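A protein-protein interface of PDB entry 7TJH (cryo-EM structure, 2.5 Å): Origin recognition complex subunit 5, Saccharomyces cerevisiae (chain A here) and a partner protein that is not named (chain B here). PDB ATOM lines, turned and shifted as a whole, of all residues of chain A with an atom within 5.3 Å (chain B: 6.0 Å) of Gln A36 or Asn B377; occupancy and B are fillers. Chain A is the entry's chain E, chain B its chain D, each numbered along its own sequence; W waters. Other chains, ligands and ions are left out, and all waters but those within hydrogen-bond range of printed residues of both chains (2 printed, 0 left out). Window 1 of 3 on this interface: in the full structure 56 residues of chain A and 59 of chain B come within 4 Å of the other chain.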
ATOM      1  N   ILE A  34      18.359  11.940  -9.393  1.00  0.00           N
ATOM      2  CA  ILE A  34      18.746  10.693 -10.045  1.00  0.00           C
ATOM      3  C   ILE A  34      19.074   9.662  -8.973  1.00  0.00           C
ATOM      4  O   ILE A  34      19.793   9.966  -8.016  1.00  0.00           O
ATOM      5  CB  ILE A  34      19.935  10.902 -11.004  1.00  0.00           C
ATOM      6  CG1 ILE A  34      19.528  11.826 -12.151  1.00  0.00           C
ATOM      7  CG2 ILE A  34      20.435   9.579 -11.569  1.00  0.00           C
ATOM      8  CD1 ILE A  34      20.665  12.208 -13.060  1.00  0.00           C
ATOM      9  N   LEU A  35      18.502   8.468  -9.106  1.00  0.00           N
ATOM     10  CA  LEU A  35      18.914   7.292  -8.351  1.00  0.00           C
ATOM     11  C   LEU A  35      19.668   6.385  -9.310  1.00  0.00           C
ATOM     12  O   LEU A  35      19.133   6.007 -10.353  1.00  0.00           O
ATOM     13  CB  LEU A  35      17.717   6.553  -7.750  1.00  0.00           C
ATOM     14  CG  LEU A  35      17.006   6.998  -6.467  1.00  0.00           C
ATOM     15  CD1 LEU A  35      16.350   8.360  -6.572  1.00  0.00           C
ATOM     16  CD2 LEU A  35      15.985   5.946  -6.052  1.00  0.00           C
ATOM     17  N   GLN A  36      20.908   6.045  -8.986  1.00  0.00           N
ATOM     18  CA  GLN A  36      21.696   5.228  -9.898  1.00  0.00           C
ATOM     19  C   GLN A  36      22.200   3.989  -9.182  1.00  0.00           C
ATOM     20  O   GLN A  36      22.844   4.091  -8.138  1.00  0.00           O
ATOM     21  CB  GLN A  36      22.869   6.012 -10.494  1.00  0.00           C
ATOM     22  CG  GLN A  36      23.570   5.286 -11.631  1.00  0.00           C
ATOM     23  CD  GLN A  36      24.777   4.497 -11.164  1.00  0.00           C
ATOM     24  OE1 GLN A  36      25.566   4.976 -10.356  1.00  0.00           O
ATOM     25  NE2 GLN A  36      24.914   3.273 -11.656  1.00  0.00           N
ATOM     26  N   GLY A  37      21.927   2.834  -9.765  1.00  0.00           N
ATOM     27  CA  GLY A  37      22.424   1.578  -9.242  1.00  0.00           C
ATOM     28  C   GLY A  37      22.147   0.477 -10.234  1.00  0.00           C
ATOM     29  O   GLY A  37      21.265   0.592 -11.089  1.00  0.00           O
ATOM     30  N   TYR A  38      22.901  -0.604 -10.103  1.00  0.00           N
ATOM     31  CA  TYR A  38      22.717  -1.722 -11.012  1.00  0.00           C
ATOM     32  C   TYR A  38      21.537  -2.572 -10.549  1.00  0.00           C
ATOM     33  O   TYR A  38      20.812  -2.216  -9.616  1.00  0.00           O
ATOM     34  CB  TYR A  38      24.019  -2.508 -11.147  1.00  0.00           C
ATOM     35  CG  TYR A  38      25.045  -1.724 -11.933  1.00  0.00           C
ATOM     36  CD1 TYR A  38      25.121  -1.837 -13.314  1.00  0.00           C
ATOM     37  CD2 TYR A  38      25.907  -0.836 -11.297  1.00  0.00           C
ATOM     38  CE1 TYR A  38      26.042  -1.107 -14.039  1.00  0.00           C
ATOM     39  CE2 TYR A  38      26.821  -0.097 -12.010  1.00  0.00           C
ATOM     40  CZ  TYR A  38      26.889  -0.238 -13.381  1.00  0.00           C
ATOM     41  OH  TYR A  38      27.810   0.493 -14.091  1.00  0.00           O
ATOM     42  N   LYS A  43      16.690  -0.021  -5.235  1.00  0.00           N
ATOM     43  CA  LYS A  43      16.375   1.376  -5.595  1.00  0.00           C
ATOM     44  C   LYS A  43      14.875   1.564  -5.576  1.00  0.00           C
ATOM     45  O   LYS A  43      14.437   2.462  -4.917  1.00  0.00           O
ATOM     46  CB  LYS A  43      16.885   1.627  -7.019  1.00  0.00           C
ATOM     47  CG  LYS A  43      18.372   1.488  -7.279  1.00  0.00           C
ATOM     48  CD  LYS A  43      18.785   2.083  -8.610  1.00  0.00           C
ATOM     49  CE  LYS A  43      18.081   1.480  -9.807  1.00  0.00           C
ATOM     50  NZ  LYS A  43      18.450   0.068 -10.050  1.00  0.00           N
ATOM     51  N   MET A 170      18.451   5.188 -12.930  1.00  0.00           N
ATOM     52  CA  MET A 170      19.345   4.740 -13.983  1.00  0.00           C
ATOM     53  C   MET A 170      20.039   3.458 -13.562  1.00  0.00           C
ATOM     54  O   MET A 170      20.247   3.203 -12.374  1.00  0.00           O
ATOM     55  CB  MET A 170      20.407   5.787 -14.318  1.00  0.00           C
ATOM     56  CG  MET A 170      19.894   6.980 -15.068  1.00  0.00           C
ATOM     57  SD  MET A 170      21.102   8.302 -15.034  1.00  0.00           S
ATOM     58  CE  MET A 170      20.163   9.585 -15.827  1.00  0.00           C
ATOM     59  N   LEU A 171      20.408   2.657 -14.555  1.00  0.00           N
ATOM     60  CA  LEU A 171      21.136   1.427 -14.288  1.00  0.00           C
ATOM     61  C   LEU A 171      22.643   1.613 -14.428  1.00  0.00           C
ATOM     62  O   LEU A 171      23.397   1.289 -13.506  1.00  0.00           O
ATOM     63  CB  LEU A 171      20.645   0.312 -15.219  1.00  0.00           C
ATOM     64  CG  LEU A 171      19.475  -0.511 -14.678  1.00  0.00           C
ATOM     65  CD1 LEU A 171      18.798  -1.299 -15.792  1.00  0.00           C
ATOM     66  CD2 LEU A 171      19.926  -1.432 -13.565  1.00  0.00           C
ATOM     67  N   GLU A 172      23.095   2.150 -15.555  1.00  0.00           N
ATOM     68  CA  GLU A 172      24.501   2.098 -15.931  1.00  0.00           C
ATOM     69  C   GLU A 172      25.226   3.395 -15.590  1.00  0.00           C
ATOM     70  O   GLU A 172      24.661   4.487 -15.696  1.00  0.00           O
ATOM     71  CB  GLU A 172      24.648   1.792 -17.423  1.00  0.00           C
ATOM     72  CG  GLU A 172      24.268   0.362 -17.775  1.00  0.00           C
ATOM     73  CD  GLU A 172      24.030   0.152 -19.258  1.00  0.00           C
ATOM     74  OE1 GLU A 172      24.692   0.824 -20.076  1.00  0.00           O
ATOM     75  OE2 GLU A 172      23.181  -0.694 -19.606  1.00  0.00           O
ATOM     76  N   THR A 173      26.487   3.252 -15.180  1.00  0.00           N
ATOM     77  CA  THR A 173      27.304   4.399 -14.792  1.00  0.00           C
ATOM     78  C   THR A 173      27.646   5.288 -15.985  1.00  0.00           C
ATOM     79  O   THR A 173      27.664   6.514 -15.852  1.00  0.00           O
ATOM     80  CB  THR A 173      28.575   3.908 -14.089  1.00  0.00           C
ATOM     81  OG1 THR A 173      28.221   2.995 -13.045  1.00  0.00           O
ATOM     82  CG2 THR A 173      29.364   5.057 -13.484  1.00  0.00           C
ATOM     83  N   LEU A 176      24.991   7.754 -16.983  1.00  0.00           N
ATOM     84  CA  LEU A 176      24.936   8.846 -16.016  1.00  0.00           C
ATOM     85  C   LEU A 176      26.112   9.803 -16.188  1.00  0.00           C
ATOM     86  O   LEU A 176      25.948  11.025 -16.085  1.00  0.00           O
ATOM     87  CB  LEU A 176      24.896   8.282 -14.595  1.00  0.00           C
ATOM     88  CG  LEU A 176      25.032   9.282 -13.443  1.00  0.00           C
ATOM     89  CD1 LEU A 176      23.837  10.211 -13.402  1.00  0.00           C
ATOM     90  CD2 LEU A 176      25.214   8.578 -12.110  1.00  0.00           C
ATOM     91  N   THR A 186      22.432  13.241  -7.254  1.00  0.00           N
ATOM     92  CA  THR A 186      22.435  11.812  -7.518  1.00  0.00           C
ATOM     93  C   THR A 186      22.627  11.063  -6.209  1.00  0.00           C
ATOM     94  O   THR A 186      23.415  11.474  -5.355  1.00  0.00           O
ATOM     95  CB  THR A 186      23.547  11.429  -8.509  1.00  0.00           C
ATOM     96  OG1 THR A 186      23.623  12.412  -9.545  1.00  0.00           O
ATOM     97  CG2 THR A 186      23.267  10.080  -9.142  1.00  0.00           C
ATOM     98  N   VAL A 187      21.881   9.978  -6.055  1.00  0.00           N
ATOM     99  CA  VAL A 187      22.037   9.038  -4.954  1.00  0.00           C
ATOM    100  C   VAL A 187      22.449   7.709  -5.565  1.00  0.00           C
ATOM    101  O   VAL A 187      21.738   7.164  -6.420  1.00  0.00           O
ATOM    102  CB  VAL A 187      20.745   8.892  -4.135  1.00  0.00           C
ATOM    103  CG1 VAL A 187      20.979   8.005  -2.926  1.00  0.00           C
ATOM    104  CG2 VAL A 187      20.218  10.258  -3.713  1.00  0.00           C
ATOM    105  N   MET A 188      23.594   7.194  -5.144  1.00  0.00           N
ATOM    106  CA  MET A 188      24.091   5.938  -5.677  1.00  0.00           C
ATOM    107  C   MET A 188      23.694   4.776  -4.780  1.00  0.00           C
ATOM    108  O   MET A 188      23.565   4.910  -3.562  1.00  0.00           O
ATOM    109  CB  MET A 188      25.607   5.964  -5.857  1.00  0.00           C
ATOM    110  CG  MET A 188      26.059   6.635  -7.134  1.00  0.00           C
ATOM    111  SD  MET A 188      25.854   8.422  -7.094  1.00  0.00           S
ATOM    112  CE  MET A 188      26.870   8.903  -8.483  1.00  0.00           C
ATOM    113  N   PHE A 189      23.495   3.628  -5.419  1.00  0.00           N
ATOM    114  CA  PHE A 189      23.046   2.394  -4.786  1.00  0.00           C
ATOM    115  C   PHE A 189      24.090   1.341  -5.119  1.00  0.00           C
ATOM    116  O   PHE A 189      23.983   0.658  -6.148  1.00  0.00           O
ATOM    117  CB  PHE A 189      21.666   1.984  -5.287  1.00  0.00           C
ATOM    118  CG  PHE A 189      20.559   2.797  -4.713  1.00  0.00           C
ATOM    119  CD1 PHE A 189      20.303   4.086  -5.169  1.00  0.00           C
ATOM    120  CD2 PHE A 189      19.778   2.280  -3.707  1.00  0.00           C
ATOM    121  CE1 PHE A 189      19.286   4.834  -4.624  1.00  0.00           C
ATOM    122  CE2 PHE A 189      18.772   3.014  -3.167  1.00  0.00           C
ATOM    123  CZ  PHE A 189      18.516   4.297  -3.622  1.00  0.00           C
ATOM    124  N   PRO A 190      25.135   1.211  -4.307  1.00  0.00           N
ATOM    125  CA  PRO A 190      26.148   0.188  -4.577  1.00  0.00           C
ATOM    126  C   PRO A 190      25.587  -1.205  -4.352  1.00  0.00           C
ATOM    127  O   PRO A 190      24.615  -1.396  -3.617  1.00  0.00           O
ATOM    128  CB  PRO A 190      27.262   0.513  -3.578  1.00  0.00           C
ATOM    129  CG  PRO A 190      26.606   1.289  -2.504  1.00  0.00           C
ATOM    130  CD  PRO A 190      25.407   1.966  -3.074  1.00  0.00           C
ATOM    131  N   ARG A 191      26.192  -2.172  -5.037  1.00  0.00           N
ATOM    132  CA  ARG A 191      25.755  -3.556  -4.945  1.00  0.00           C
ATOM    133  C   ARG A 191      25.983  -4.101  -3.543  1.00  0.00           C
ATOM    134  O   ARG A 191      26.956  -3.747  -2.873  1.00  0.00           O
ATOM    135  CB  ARG A 191      26.493  -4.410  -5.974  1.00  0.00           C
ATOM    136  CG  ARG A 191      26.330  -3.917  -7.393  1.00  0.00           C
ATOM    137  CD  ARG A 191      26.988  -4.843  -8.387  1.00  0.00           C
ATOM    138  NE  ARG A 191      26.143  -5.988  -8.706  1.00  0.00           N
ATOM    139  CZ  ARG A 191      26.592  -7.220  -8.899  1.00  0.00           C
ATOM    140  NH1 ARG A 191      27.880  -7.506  -8.817  1.00  0.00           N
ATOM    141  NH2 ARG A 191      25.728  -8.187  -9.187  1.00  0.00           N
ATOM    142  N   ASN B 373      30.029   7.861  -1.555  1.00  0.00           N
ATOM    143  CA  ASN B 373      28.852   7.339  -2.245  1.00  0.00           C
ATOM    144  C   ASN B 373      28.842   7.713  -3.723  1.00  0.00           C
ATOM    145  O   ASN B 373      28.416   6.910  -4.559  1.00  0.00           O
ATOM    146  CB  ASN B 373      27.574   7.828  -1.571  1.00  0.00           C
ATOM    147  CG  ASN B 373      26.321   7.343  -2.283  1.00  0.00           C
ATOM    148  OD1 ASN B 373      25.727   8.069  -3.075  1.00  0.00           O
ATOM    149  ND2 ASN B 373      25.916   6.116  -1.996  1.00  0.00           N
ATOM    150  N   GLN B 374      29.311   8.920  -4.071  1.00  0.00           N
ATOM    151  CA  GLN B 374      29.334   9.333  -5.475  1.00  0.00           C
ATOM    152  C   GLN B 374      30.305   8.512  -6.320  1.00  0.00           C
ATOM    153  O   GLN B 374      30.154   8.473  -7.543  1.00  0.00           O
ATOM    154  CB  GLN B 374      29.694  10.817  -5.611  1.00  0.00           C
ATOM    155  CG  GLN B 374      28.680  11.798  -5.044  1.00  0.00           C
ATOM    156  CD  GLN B 374      27.324  11.734  -5.716  1.00  0.00           C
ATOM    157  OE1 GLN B 374      26.314  11.488  -5.066  1.00  0.00           O
ATOM    158  NE2 GLN B 374      27.293  11.977  -7.019  1.00  0.00           N
ATOM    159  N   LEU B 375      31.290   7.864  -5.701  1.00  0.00           N
ATOM    160  CA  LEU B 375      32.241   7.014  -6.401  1.00  0.00           C
ATOM    161  C   LEU B 375      31.951   5.527  -6.235  1.00  0.00           C
ATOM    162  O   LEU B 375      32.790   4.706  -6.605  1.00  0.00           O
ATOM    163  CB  LEU B 375      33.665   7.304  -5.920  1.00  0.00           C
ATOM    164  CG  LEU B 375      34.152   8.751  -5.943  1.00  0.00           C
ATOM    165  CD1 LEU B 375      35.302   8.932  -4.970  1.00  0.00           C
ATOM    166  CD2 LEU B 375      34.558   9.145  -7.346  1.00  0.00           C
ATOM    167  N   SER B 376      30.801   5.156  -5.673  1.00  0.00           N
ATOM    168  CA  SER B 376      30.592   3.762  -5.300  1.00  0.00           C
ATOM    169  C   SER B 376      30.283   2.852  -6.486  1.00  0.00           C
ATOM    170  O   SER B 376      30.557   1.652  -6.408  1.00  0.00           O
ATOM    171  CB  SER B 376      29.473   3.654  -4.261  1.00  0.00           C
ATOM    172  OG  SER B 376      28.264   4.210  -4.737  1.00  0.00           O
ATOM    173  N   ASN B 377      29.736   3.383  -7.576  1.00  0.00           N
ATOM    174  CA  ASN B 377      29.358   2.569  -8.723  1.00  0.00           C
ATOM    175  C   ASN B 377      30.314   2.699  -9.901  1.00  0.00           C
ATOM    176  O   ASN B 377      29.966   2.278 -11.006  1.00  0.00           O
ATOM    177  CB  ASN B 377      27.932   2.906  -9.171  1.00  0.00           C
ATOM    178  CG  ASN B 377      26.879   2.318  -8.254  1.00  0.00           C
ATOM    179  OD1 ASN B 377      27.105   1.292  -7.616  1.00  0.00           O
ATOM    180  ND2 ASN B 377      25.719   2.960  -8.187  1.00  0.00           N
ATOM    181  N   ASN B 378      31.510   3.247  -9.705  1.00  0.00           N
ATOM    182  CA  ASN B 378      32.458   3.361 -10.809  1.00  0.00           C
ATOM    183  C   ASN B 378      33.193   2.027 -11.001  1.00  0.00           C
ATOM    184  O   ASN B 378      32.818   1.002 -10.427  1.00  0.00           O
ATOM    185  CB  ASN B 378      33.382   4.567 -10.603  1.00  0.00           C
ATOM    186  CG  ASN B 378      34.270   4.475  -9.356  1.00  0.00           C
ATOM    187  OD1 ASN B 378      34.328   3.468  -8.650  1.00  0.00           O
ATOM    188  ND2 ASN B 378      34.964   5.567  -9.081  1.00  0.00           N
ATOM    189  N   LEU B 379      34.246   2.032 -11.826  1.00  0.00           N
ATOM    190  CA  LEU B 379      34.974   0.800 -12.136  1.00  0.00           C
ATOM    191  C   LEU B 379      35.665   0.220 -10.906  1.00  0.00           C
ATOM    192  O   LEU B 379      35.690  -1.003 -10.723  1.00  0.00           O
ATOM    193  CB  LEU B 379      35.990   1.054 -13.247  1.00  0.00           C
ATOM    194  CG  LEU B 379      35.439   0.985 -14.672  1.00  0.00           C
ATOM    195  CD1 LEU B 379      36.381   1.667 -15.650  1.00  0.00           C
ATOM    196  CD2 LEU B 379      35.196  -0.459 -15.077  1.00  0.00           C
ATOM    197  N   GLY B 381      34.711   0.660  -7.677  1.00  0.00           N
ATOM    198  CA  GLY B 381      33.727   0.164  -6.732  1.00  0.00           C
ATOM    199  C   GLY B 381      32.967  -1.052  -7.210  1.00  0.00           C
ATOM    200  O   GLY B 381      32.552  -1.881  -6.396  1.00  0.00           O
ATOM    201  N   ARG B 382      32.763  -1.172  -8.524  1.00  0.00           N
ATOM    202  CA  ARG B 382      32.112  -2.352  -9.080  1.00  0.00           C
ATOM    203  C   ARG B 382      32.992  -3.589  -8.979  1.00  0.00           C
ATOM    204  O   ARG B 382      32.470  -4.706  -8.894  1.00  0.00           O
ATOM    205  CB  ARG B 382      31.740  -2.111 -10.538  1.00  0.00           C
ATOM    206  CG  ARG B 382      30.310  -1.706 -10.771  1.00  0.00           C
ATOM    207  CD  ARG B 382      30.100  -1.442 -12.238  1.00  0.00           C
ATOM    208  NE  ARG B 382      30.499  -0.084 -12.579  1.00  0.00           N
ATOM    209  CZ  ARG B 382      31.093   0.261 -13.711  1.00  0.00           C
ATOM    210  NH1 ARG B 382      31.377  -0.632 -14.643  1.00  0.00           N
ATOM    211  NH2 ARG B 382      31.413   1.535 -13.912  1.00  0.00           N
HETATM  212  O   HOH W   1      24.883  -0.720  -8.170  1.00  0.00           O
HETATM  213  O   HOH W   2      28.691  -0.988  -7.016  1.00  0.00           O
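O of Met A188 lies within hydrogen-bond range of ND2 of Asn B373, at 3.1 Å.
OE1 of Gln B374 lies close to O of Thr A186, at 2.9 Å.
The side-chain amide oxygen of Gln B374 sits close to the side-chain sulfur of Met A188.
The side-chain amide oxygen (OE1) of Gln A36 sits at hydrogen-bond distance from the side-chain amide nitrogen (ND2) of Asn B377 (3.0 Å).
The backbone carbonyl oxygen of Asn B377 sits at hydrogen-bond distance from the side-chain hydroxyl of Thr A173, at 2.8 Å.
The side-chain hydroxyl (OH) of Tyr A38 sits at hydrogen-bond distance from the guanidinium group (NE) of Arg B382 (3.1 Å).
The side-chain hydroxyl (OG) of Ser B376 lies within hydrogen-bond range of the backbone carbonyl oxygen (O) of Asn B373 (2.7 Å).
The backbone carbonyl oxygen (O) of Asn B378 sits close to the guanidinium group (NE) of Arg B382 (3.3 Å).
O of Val A187 is in hydrogen-bond range of N of Gln A36 (2.9 Å).
The backbone NH (N) of Phe A189 is in hydrogen-bond range of the backbone carbonyl oxygen (O) of Gln A36 (2.8 Å).
The backbone carbonyl oxygen of Gly A37 is in hydrogen-bond range of the side-chain amino group of Lys A43 (3.0 Å).
O of Tyr A38 sits at hydrogen-bond distance from NZ of Lys A43 (3.3 Å).
Gly A37 touches Asn B377 (CA to ND2, 3.7 Å).
OG1 of Thr A173 touches NH2 of Arg B382, 3.6 Å away.
Met A188 touches Ser B376 (CB to OG, 3.4 Å).
CB of Met A188 touches ND2 of Asn B377, at 3.8 Å.
Asn B377 touches Phe A189 (OD1 to O, 3.5 Å).
Ser B376 touches Pro A190 (CB to CB, 3.9 Å).
Pro A190 touches Asn B377 (CA to OD1, 3.4 Å).
Of chain B, only Asn B377 (3.0 Å) comes within 4 Å of Gln A36.
Asn B377 touches just these residues of chain A: Gln A36 (3.0 Å), Gly A37 (3.7 Å), Thr A173 (2.8 Å), Met A188 (3.8 Å), Phe A189 (3.5 Å) and Pro A190 (3.4 Å).
Printed residues of chain A within 4 Å of Arg B382: Tyr A38 and Thr A173.
Of the printed residues of chain B, Phe A189 touches Asn B377.
Of the printed residues of chain B, Gly A37 touches Asn B377 (3.7 Å).
Of the printed residues of chain B, Tyr A38 touches Arg B382.
Printed residues of chain B within 4 Å of Met A188: Asn B373, Gln B374, Ser B376 and Asn B377.
Val A187 touches none of the printed residues of chain B.
Leu B379 touches none of the printed residues of chain A.
The nearest printed residue of chain B that does not touch Gln A36 is Asn B378 (6.2 Å).
The nearest printed residue of chain A that does not touch Gln B374 is Val A187 (4.8 Å).
Hydrophobic or aromatic side chains of chain A that line the printed part of chain B: Tyr A38, Met A188 and Pro A190.
Of the 9 printed residues of chain B, 5 touch a printed residue of chain A.
Water W1 lies within hydrogen-bond range of O of Phe A189, N of Tyr A38 and OD1 of Asn B377.
Water W2 lies within hydrogen-bond range of OD1 of Asn B377 (2.8 Å), O of Ser B376 (3.3 Å) and N of Arg A191 (3.4 Å).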
